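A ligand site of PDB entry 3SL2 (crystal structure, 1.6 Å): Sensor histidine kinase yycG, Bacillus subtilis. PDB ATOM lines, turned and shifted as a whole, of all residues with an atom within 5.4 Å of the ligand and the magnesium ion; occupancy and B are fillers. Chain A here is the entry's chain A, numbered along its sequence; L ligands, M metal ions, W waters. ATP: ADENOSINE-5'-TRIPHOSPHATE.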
ATOM      1  N   ASN A  50       0.016 -15.420 -13.391  1.00  0.00           N
ATOM      2  CA  ASN A  50      -0.545 -16.761 -13.464  1.00  0.00           C
ATOM      3  C   ASN A  50       0.128 -17.590 -14.518  1.00  0.00           C
ATOM      4  O   ASN A  50       0.382 -18.771 -14.291  1.00  0.00           O
ATOM      5  CB  ASN A  50      -2.067 -16.727 -13.682  1.00  0.00           C
ATOM      6  CG  ASN A  50      -2.830 -16.186 -12.461  1.00  0.00           C
ATOM      7  OD1 ASN A  50      -2.228 -15.835 -11.432  1.00  0.00           O
ATOM      8  ND2 ASN A  50      -4.128 -16.126 -12.569  1.00  0.00           N
ATOM      9  N   SER A  53       3.778 -18.167 -13.312  1.00  0.00           N
ATOM     10  CA  SER A  53       3.772 -19.151 -12.218  1.00  0.00           C
ATOM     11  C   SER A  53       3.734 -20.569 -12.785  1.00  0.00           C
ATOM     12  O   SER A  53       4.473 -21.459 -12.328  1.00  0.00           O
ATOM     13  CB  SER A  53       2.578 -18.896 -11.295  1.00  0.00           C
ATOM     14  OG  SER A  53       2.149 -20.085 -10.643  1.00  0.00           O
ATOM     15  N   ASN A  54       2.897 -20.786 -13.796  1.00  0.00           N
ATOM     16  CA  ASN A  54       2.823 -22.081 -14.463  1.00  0.00           C
ATOM     17  C   ASN A  54       4.129 -22.464 -15.159  1.00  0.00           C
ATOM     18  O   ASN A  54       4.594 -23.582 -15.040  1.00  0.00           O
ATOM     19  CB  ASN A  54       1.678 -22.141 -15.466  1.00  0.00           C
ATOM     20  CG  ASN A  54       0.299 -22.126 -14.812  1.00  0.00           C
ATOM     21  OD1 ASN A  54       0.120 -22.418 -13.607  1.00  0.00           O
ATOM     22  ND2 ASN A  54      -0.695 -21.757 -15.614  1.00  0.00           N
ATOM     23  N   ALA A  55       4.698 -21.531 -15.917  1.00  0.00           N
ATOM     24  CA  ALA A  55       5.916 -21.807 -16.654  1.00  0.00           C
ATOM     25  C   ALA A  55       7.022 -22.258 -15.722  1.00  0.00           C
ATOM     26  O   ALA A  55       7.742 -23.197 -16.048  1.00  0.00           O
ATOM     27  CB  ALA A  55       6.347 -20.579 -17.453  1.00  0.00           C
ATOM     28  N   LYS A  57       6.567 -23.399 -12.436  1.00  0.00           N
ATOM     29  CA  LYS A  57       6.075 -24.584 -11.717  1.00  0.00           C
ATOM     30  C   LYS A  57       6.316 -25.859 -12.510  1.00  0.00           C
ATOM     31  O   LYS A  57       6.661 -26.899 -11.934  1.00  0.00           O
ATOM     32  CB  LYS A  57       4.578 -24.424 -11.447  1.00  0.00           C
ATOM     33  CG  LYS A  57       3.933 -25.392 -10.475  1.00  0.00           C
ATOM     34  CD  LYS A  57       2.485 -24.990 -10.247  1.00  0.00           C
ATOM     35  CE  LYS A  57       1.804 -25.766  -9.123  1.00  0.00           C
ATOM     36  NZ  LYS A  57       0.377 -25.317  -9.001  1.00  0.00           N
ATOM     37  N   TYR A  58       6.177 -25.766 -13.838  1.00  0.00           N
ATOM     38  CA  TYR A  58       6.210 -26.930 -14.710  1.00  0.00           C
ATOM     39  C   TYR A  58       7.496 -27.040 -15.537  1.00  0.00           C
ATOM     40  O   TYR A  58       7.558 -27.853 -16.458  1.00  0.00           O
ATOM     41  CB  TYR A  58       4.937 -26.955 -15.604  1.00  0.00           C
ATOM     42  CG  TYR A  58       3.635 -26.975 -14.819  1.00  0.00           C
ATOM     43  CD1 TYR A  58       3.282 -28.075 -14.024  1.00  0.00           C
ATOM     44  CD2 TYR A  58       2.758 -25.901 -14.856  1.00  0.00           C
ATOM     45  CE1 TYR A  58       2.092 -28.082 -13.295  1.00  0.00           C
ATOM     46  CE2 TYR A  58       1.578 -25.900 -14.138  1.00  0.00           C
ATOM     47  CZ  TYR A  58       1.246 -27.001 -13.361  1.00  0.00           C
ATOM     48  OH  TYR A  58       0.065 -26.989 -12.645  1.00  0.00           O
ATOM     49  N   ASP A  84       7.971 -21.963 -22.438  1.00  0.00           N
ATOM     50  CA  ASP A  84       8.809 -22.754 -21.514  1.00  0.00           C
ATOM     51  C   ASP A  84       9.267 -24.034 -22.201  1.00  0.00           C
ATOM     52  O   ASP A  84       8.779 -24.394 -23.292  1.00  0.00           O
ATOM     53  CB  ASP A  84       8.040 -23.023 -20.205  1.00  0.00           C
ATOM     54  CG  ASP A  84       6.862 -23.967 -20.383  1.00  0.00           C
ATOM     55  OD1 ASP A  84       7.072 -25.115 -20.781  1.00  0.00           O
ATOM     56  OD2 ASP A  84       5.715 -23.588 -20.082  1.00  0.00           O
ATOM     57  N   ILE A  87       7.355 -29.726 -19.004  1.00  0.00           N
ATOM     58  CA  ILE A  87       6.727 -31.017 -19.250  1.00  0.00           C
ATOM     59  C   ILE A  87       5.738 -31.038 -20.420  1.00  0.00           C
ATOM     60  O   ILE A  87       5.483 -32.089 -20.982  1.00  0.00           O
ATOM     61  CB  ILE A  87       6.070 -31.604 -17.970  1.00  0.00           C
ATOM     62  CG1 ILE A  87       4.979 -30.674 -17.411  1.00  0.00           C
ATOM     63  CG2 ILE A  87       7.138 -31.919 -16.918  1.00  0.00           C
ATOM     64  CD1 ILE A  87       4.138 -31.346 -16.312  1.00  0.00           C
ATOM     65  N   GLY A  88       5.199 -29.870 -20.774  1.00  0.00           N
ATOM     66  CA  GLY A  88       4.258 -29.797 -21.884  1.00  0.00           C
ATOM     67  C   GLY A  88       2.877 -30.277 -21.483  1.00  0.00           C
ATOM     68  O   GLY A  88       2.630 -30.570 -20.312  1.00  0.00           O
ATOM     69  N   ILE A  89       1.975 -30.352 -22.458  1.00  0.00           N
ATOM     70  CA  ILE A  89       0.578 -30.694 -22.210  1.00  0.00           C
ATOM     71  C   ILE A  89       0.102 -31.731 -23.223  1.00  0.00           C
ATOM     72  O   ILE A  89       0.323 -31.566 -24.418  1.00  0.00           O
ATOM     73  CB  ILE A  89      -0.317 -29.422 -22.266  1.00  0.00           C
ATOM     74  CG1 ILE A  89       0.228 -28.346 -21.306  1.00  0.00           C
ATOM     75  CG2 ILE A  89      -1.778 -29.767 -21.931  1.00  0.00           C
ATOM     76  CD1 ILE A  89      -0.451 -26.993 -21.422  1.00  0.00           C
ATOM     77  N   VAL A  97      -7.147 -26.531 -20.903  1.00  0.00           N
ATOM     78  CA  VAL A  97      -6.355 -26.008 -19.786  1.00  0.00           C
ATOM     79  C   VAL A  97      -6.851 -24.664 -19.262  1.00  0.00           C
ATOM     80  O   VAL A  97      -6.538 -24.293 -18.123  1.00  0.00           O
ATOM     81  CB  VAL A  97      -4.826 -26.007 -20.018  1.00  0.00           C
ATOM     82  CG1 VAL A  97      -4.289 -27.493 -20.023  1.00  0.00           C
ATOM     83  CG2 VAL A  97      -4.453 -25.198 -21.276  1.00  0.00           C
ATOM     84  N   TYR A 102      -9.957 -27.089 -14.281  1.00  0.00           N
ATOM     85  CA  TYR A 102      -9.287 -28.129 -15.052  1.00  0.00           C
ATOM     86  C   TYR A 102      -7.794 -28.215 -14.756  1.00  0.00           C
ATOM     87  O   TYR A 102      -7.062 -27.217 -14.836  1.00  0.00           O
ATOM     88  CB  TYR A 102      -9.559 -28.018 -16.582  1.00  0.00           C
ATOM     89  CG  TYR A 102      -8.929 -29.187 -17.306  1.00  0.00           C
ATOM     90  CD1 TYR A 102      -7.606 -29.126 -17.761  1.00  0.00           C
ATOM     91  CD2 TYR A 102      -9.629 -30.399 -17.457  1.00  0.00           C
ATOM     92  CE1 TYR A 102      -7.008 -30.222 -18.386  1.00  0.00           C
ATOM     93  CE2 TYR A 102      -9.030 -31.506 -18.090  1.00  0.00           C
ATOM     94  CZ  TYR A 102      -7.732 -31.397 -18.544  1.00  0.00           C
ATOM     95  OH  TYR A 102      -7.126 -32.481 -19.160  1.00  0.00           O
ATOM     96  N   ARG A 103      -7.354 -29.424 -14.352  1.00  0.00           N
ATOM     97  CA  ARG A 103      -5.940 -29.747 -14.240  1.00  0.00           C
ATOM     98  C   ARG A 103      -5.629 -31.025 -15.028  1.00  0.00           C
ATOM     99  O   ARG A 103      -6.454 -31.929 -15.079  1.00  0.00           O
ATOM    100  CB  ARG A 103      -5.569 -29.937 -12.753  1.00  0.00           C
ATOM    101  CG  ARG A 103      -5.760 -28.688 -11.892  1.00  0.00           C
ATOM    102  CD  ARG A 103      -5.214 -28.876 -10.496  1.00  0.00           C
ATOM    103  NE  ARG A 103      -5.834 -30.037  -9.879  1.00  0.00           N
ATOM    104  CZ  ARG A 103      -5.190 -30.922  -9.125  1.00  0.00           C
ATOM    105  NH1 ARG A 103      -3.889 -30.768  -8.876  1.00  0.00           N
ATOM    106  NH2 ARG A 103      -5.847 -31.961  -8.620  1.00  0.00           N
ATOM    107  N   VAL A 104      -4.435 -31.127 -15.609  1.00  0.00           N
ATOM    108  CA  VAL A 104      -4.111 -32.318 -16.429  1.00  0.00           C
ATOM    109  C   VAL A 104      -4.195 -33.612 -15.599  1.00  0.00           C
ATOM    110  O   VAL A 104      -4.644 -34.653 -16.114  1.00  0.00           O
ATOM    111  CB  VAL A 104      -2.762 -32.185 -17.166  1.00  0.00           C
ATOM    112  CG1 VAL A 104      -2.323 -33.515 -17.767  1.00  0.00           C
ATOM    113  CG2 VAL A 104      -2.894 -31.123 -18.259  1.00  0.00           C
ATOM    114  N   ASP A 105      -3.808 -33.549 -14.330  1.00  0.00           N
ATOM    115  CA  ASP A 105      -4.060 -34.698 -13.450  1.00  0.00           C
ATOM    116  C   ASP A 105      -4.718 -34.355 -12.122  1.00  0.00           C
ATOM    117  O   ASP A 105      -4.266 -33.445 -11.407  1.00  0.00           O
ATOM    118  CB  ASP A 105      -2.782 -35.520 -13.264  1.00  0.00           C
ATOM    119  CG  ASP A 105      -2.581 -36.549 -14.358  1.00  0.00           C
ATOM    120  OD1 ASP A 105      -3.112 -37.672 -14.217  1.00  0.00           O
ATOM    121  OD2 ASP A 105      -1.902 -36.223 -15.366  1.00  0.00           O
ATOM    122  N   GLY A 114      -5.376 -29.528  -6.089  1.00  0.00           N
ATOM    123  CA  GLY A 114      -5.039 -28.241  -6.710  1.00  0.00           C
ATOM    124  C   GLY A 114      -6.255 -27.499  -7.195  1.00  0.00           C
ATOM    125  O   GLY A 114      -7.315 -28.092  -7.396  1.00  0.00           O
ATOM    126  N   THR A 115      -6.094 -26.210  -7.493  1.00  0.00           N
ATOM    127  CA  THR A 115      -7.251 -25.357  -7.748  1.00  0.00           C
ATOM    128  C   THR A 115      -7.683 -25.390  -9.196  1.00  0.00           C
ATOM    129  O   THR A 115      -8.855 -25.610  -9.489  1.00  0.00           O
ATOM    130  CB  THR A 115      -7.011 -23.922  -7.262  1.00  0.00           C
ATOM    131  OG1 THR A 115      -6.771 -23.954  -5.857  1.00  0.00           O
ATOM    132  CG2 THR A 115      -8.230 -23.061  -7.491  1.00  0.00           C
ATOM    133  N   GLY A 116      -6.719 -25.154 -10.093  1.00  0.00           N
ATOM    134  CA  GLY A 116      -6.986 -25.114 -11.563  1.00  0.00           C
ATOM    135  C   GLY A 116      -7.756 -23.895 -12.039  1.00  0.00           C
ATOM    136  O   GLY A 116      -8.539 -23.975 -12.986  1.00  0.00           O
ATOM    137  N   LEU A 117      -7.544 -22.763 -11.390  1.00  0.00           N
ATOM    138  CA  LEU A 117      -8.157 -21.507 -11.852  1.00  0.00           C
ATOM    139  C   LEU A 117      -7.199 -20.491 -12.488  1.00  0.00           C
ATOM    140  O   LEU A 117      -7.692 -19.564 -13.117  1.00  0.00           O
ATOM    141  CB  LEU A 117      -8.918 -20.852 -10.687  1.00  0.00           C
ATOM    142  CG  LEU A 117     -10.191 -21.583 -10.335  1.00  0.00           C
ATOM    143  CD1 LEU A 117     -10.733 -20.963  -9.060  1.00  0.00           C
ATOM    144  CD2 LEU A 117     -11.259 -21.559 -11.425  1.00  0.00           C
ATOM    145  N   GLY A 118      -5.875 -20.642 -12.325  1.00  0.00           N
ATOM    146  CA  GLY A 118      -4.901 -19.646 -12.835  1.00  0.00           C
ATOM    147  C   GLY A 118      -5.194 -19.258 -14.265  1.00  0.00           C
ATOM    148  O   GLY A 118      -5.274 -18.074 -14.583  1.00  0.00           O
ATOM    149  N   LEU A 119      -5.370 -20.262 -15.102  1.00  0.00           N
ATOM    150  CA  LEU A 119      -5.532 -19.965 -16.542  1.00  0.00           C
ATOM    151  C   LEU A 119      -6.951 -19.577 -16.897  1.00  0.00           C
ATOM    152  O   LEU A 119      -7.193 -18.879 -17.913  1.00  0.00           O
ATOM    153  CB  LEU A 119      -5.078 -21.136 -17.377  1.00  0.00           C
ATOM    154  CG  LEU A 119      -3.592 -21.359 -17.518  1.00  0.00           C
ATOM    155  CD1 LEU A 119      -3.406 -22.494 -18.496  1.00  0.00           C
ATOM    156  CD2 LEU A 119      -2.857 -20.081 -18.033  1.00  0.00           C
ATOM    157  N   ALA A 120      -7.907 -19.983 -16.056  1.00  0.00           N
ATOM    158  CA  ALA A 120      -9.272 -19.505 -16.248  1.00  0.00           C
ATOM    159  C   ALA A 120      -9.378 -18.021 -15.963  1.00  0.00           C
ATOM    160  O   ALA A 120     -10.071 -17.275 -16.670  1.00  0.00           O
ATOM    161  CB  ALA A 120     -10.212 -20.298 -15.350  1.00  0.00           C
ATOM    162  N   THR A 143       5.721 -25.620 -23.543  1.00  0.00           N
ATOM    163  CA  THR A 143       4.438 -24.936 -23.761  1.00  0.00           C
ATOM    164  C   THR A 143       4.671 -23.464 -24.041  1.00  0.00           C
ATOM    165  O   THR A 143       5.493 -22.815 -23.386  1.00  0.00           O
ATOM    166  CB  THR A 143       3.501 -25.097 -22.519  1.00  0.00           C
ATOM    167  OG1 THR A 143       3.311 -26.493 -22.237  1.00  0.00           O
ATOM    168  CG2 THR A 143       2.116 -24.418 -22.711  1.00  0.00           C
ATOM    169  N   ILE A 145       2.154 -20.131 -23.998  1.00  0.00           N
ATOM    170  CA  ILE A 145       0.875 -19.479 -23.825  1.00  0.00           C
ATOM    171  C   ILE A 145       0.937 -18.123 -24.504  1.00  0.00           C
ATOM    172  O   ILE A 145       1.867 -17.353 -24.255  1.00  0.00           O
ATOM    173  CB  ILE A 145       0.521 -19.252 -22.311  1.00  0.00           C
ATOM    174  CG1 ILE A 145       0.582 -20.578 -21.508  1.00  0.00           C
ATOM    175  CG2 ILE A 145      -0.858 -18.566 -22.190  1.00  0.00           C
ATOM    176  CD1 ILE A 145      -0.401 -21.645 -21.939  1.00  0.00           C
HETATM  177  PG  ATP L   1      -3.796 -22.697  -9.947  1.00  0.00           P
HETATM  178  O1G ATP L   1      -2.985 -21.916 -11.044  1.00  0.00           O
HETATM  179  O2G ATP L   1      -3.081 -22.749  -8.560  1.00  0.00           O
HETATM  180  O3G ATP L   1      -5.172 -22.252  -9.812  1.00  0.00           O
HETATM  181  PB  ATP L   1      -3.071 -24.874 -11.694  1.00  0.00           P
HETATM  182  O1B ATP L   1      -1.747 -24.226 -11.890  1.00  0.00           O
HETATM  183  O2B ATP L   1      -3.193 -26.388 -11.766  1.00  0.00           O
HETATM  184  O3B ATP L   1      -3.739 -24.187 -10.437  1.00  0.00           O
HETATM  185  PA  ATP L   1      -3.950 -23.442 -14.141  1.00  0.00           P
HETATM  186  O1A ATP L   1      -2.918 -22.403 -13.854  1.00  0.00           O
HETATM  187  O2A ATP L   1      -5.321 -22.944 -14.468  1.00  0.00           O
HETATM  188  O3A ATP L   1      -4.213 -24.310 -12.736  1.00  0.00           O
HETATM  189  O5' ATP L   1      -3.456 -24.539 -15.116  1.00  0.00           O
HETATM  190  C5' ATP L   1      -4.296 -25.664 -15.480  1.00  0.00           C
HETATM  191  C4' ATP L   1      -3.526 -26.913 -15.809  1.00  0.00           C
HETATM  192  O4' ATP L   1      -2.861 -26.730 -17.081  1.00  0.00           O
HETATM  193  C3' ATP L   1      -2.439 -27.211 -14.789  1.00  0.00           C
HETATM  194  O3' ATP L   1      -2.989 -27.898 -13.630  1.00  0.00           O
HETATM  195  C2' ATP L   1      -1.458 -28.001 -15.638  1.00  0.00           C
HETATM  196  O2' ATP L   1      -1.870 -29.367 -15.830  1.00  0.00           O
HETATM  197  C1' ATP L   1      -1.594 -27.379 -17.022  1.00  0.00           C
HETATM  198  N9  ATP L   1      -0.573 -26.349 -17.331  1.00  0.00           N
HETATM  199  C8  ATP L   1      -0.738 -25.000 -17.243  1.00  0.00           C
HETATM  200  N7  ATP L   1       0.383 -24.339 -17.635  1.00  0.00           N
HETATM  201  C5  ATP L   1       1.275 -25.286 -17.981  1.00  0.00           C
HETATM  202  C6  ATP L   1       2.658 -25.298 -18.482  1.00  0.00           C
HETATM  203  N6  ATP L   1       3.297 -24.113 -18.685  1.00  0.00           N
HETATM  204  N1  ATP L   1       3.258 -26.506 -18.706  1.00  0.00           N
HETATM  205  C2  ATP L   1       2.606 -27.670 -18.496  1.00  0.00           C
HETATM  206  N3  ATP L   1       1.334 -27.735 -18.037  1.00  0.00           N
HETATM  207  C4  ATP L   1       0.648 -26.599 -17.768  1.00  0.00           C
HETATM  208 MG    MG M   1      -1.458 -22.232 -12.302  1.00  0.00          MG
HETATM  209  O   HOH W   1      -5.897 -20.000  -8.441  1.00  0.00           O
HETATM  210  O   HOH W   2       0.049 -22.176 -10.873  1.00  0.00           O
HETATM  211  O   HOH W   3      -7.464 -24.488 -15.559  1.00  0.00           O
HETATM  212  O   HOH W   4      -1.995 -30.737 -13.321  1.00  0.00           O
HETATM  213  O   HOH W   5       5.236 -27.071 -20.478  1.00  0.00           O
HETATM  214  O   HOH W   6      -1.949 -19.052 -10.302  1.00  0.00           O
HETATM  215  O   HOH W   7      -0.589 -22.836  -8.326  1.00  0.00           O
HETATM  216  O   HOH W   8       0.259 -21.574 -18.346  1.00  0.00           O
HETATM  217  O   HOH W   9      -1.333 -20.108 -12.703  1.00  0.00           O
HETATM  218  O   HOH W  10       2.926 -21.016 -18.660  1.00  0.00           O
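O2A of the ligand sits at hydrogen-bond distance from N of Leu 119, at 2.8 Å.
The side-chain carboxylate (OD2) of Asp 84 lies within hydrogen-bond range of a nitrogen (N6) of the ligand.
N of Leu 117 lies within hydrogen-bond range of O3G of the ligand.
An oxygen (O3G) of the ligand sits at hydrogen-bond distance from the backbone NH of Gly 118, 3.1 Å away.
An oxygen (O3B) of the ligand is in hydrogen-bond range of the backbone NH (N) of Gly 116, 3.2 Å away.
O2' of the ligand lies within hydrogen-bond range of N of Val 104, 3.1 Å away.
The side-chain hydroxyl (OH) of Tyr 58 sits close to an oxygen (O3') of the ligand (3.3 Å).
The side-chain amino group (NZ) of Lys 57 lies close to an oxygen (O1B) of the ligand, 3.7 Å away.
The side-chain amide nitrogen of Asn 54 sits close to the backbone carbonyl oxygen of Asn 50 (3.4 Å).
The backbone NH (N) of Asp 84 sits at hydrogen-bond distance from the backbone carbonyl oxygen (O) of Thr 143.
The backbone carbonyl oxygen (O) of Gly 118 lies within hydrogen-bond range of the side-chain amide nitrogen (ND2) of Asn 50.
The backbone carbonyl oxygen of Tyr 58 lies within hydrogen-bond range of the backbone NH of Ile 87 (3.2 Å).
The guanidinium group (NE) of Arg 103 is in hydrogen-bond range of the backbone carbonyl oxygen (O) of Gly 114 (3.5 Å).
Ile 87 touches the ligand.
Gly 88 touches the ligand.
Ile 89 touches the ligand (CG1 to N3, 3.5 Å).
CG1 of Val 97 touches O4' of the ligand (3.4 Å).
O of Tyr 102 touches C5' of the ligand (3.2 Å).
CG of Arg 103 touches O3' of the ligand, 3.4 Å away.
Thr 115 touches the ligand (CB to O3G, 3.6 Å).
Thr 143 touches the ligand (OG1 to N1, 3.5 Å).
Hydrophobic or aromatic side chains within 4 Å of the ligand: Tyr 58, Ile 87, Ile 89, Val 97, Val 104 and Leu 119.
Of the 24 residues printed, 17 come within 4 Å of the ligand.
Along chain A the residues within 4 Å of the ligand span positions 54 to 143.
The nearest printed residue that does not touch the magnesium ion is Gly 118 (4.3 Å).
An oxygen (O1G) of the ligand is bound to the magnesium ion (2.0 Å).
OD1 of Asn 54 binds the magnesium ion (2.1 Å).
O1B of the ligand is bound to the magnesium ion.
Water W2 is bound to the magnesium ion.
O1A of the ligand is bound to the magnesium ion.
Water W9 is bound to the magnesium ion.
The magnesium ion has six donor atoms within binding distance.
Water W9 lies within hydrogen-bond range of the backbone carbonyl oxygen (O) of Asn 50 (2.7 Å) and the side-chain amide nitrogen (ND2) of Asn 54 (3.4 Å).
Water W7 bridges an oxygen (O2G) of the ligand and the side-chain amino group of Lys 57.
Water W5 lies within hydrogen-bond range of OG1 of Thr 143 (2.7 Å), OD1 of Asp 84 (2.7 Å), N1 of the ligand (2.7 Å) and N of Gly 88 (2.8 Å).
Water W8 bridges a nitrogen (N7) of the ligand (2.9 Å) and the side-chain amide nitrogen (ND2) of Asn 54 (2.9 Å).
Water W4 lies within hydrogen-bond range of an oxygen (O2') of the ligand (2.9 Å), the backbone NH of Val 104 (3.4 Å) and the backbone NH of Asp 105 (3.5 Å).
Water W10 lies within hydrogen-bond range of N6 of the ligand (3.1 Å) and N of Ala 55 (3.3 Å).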
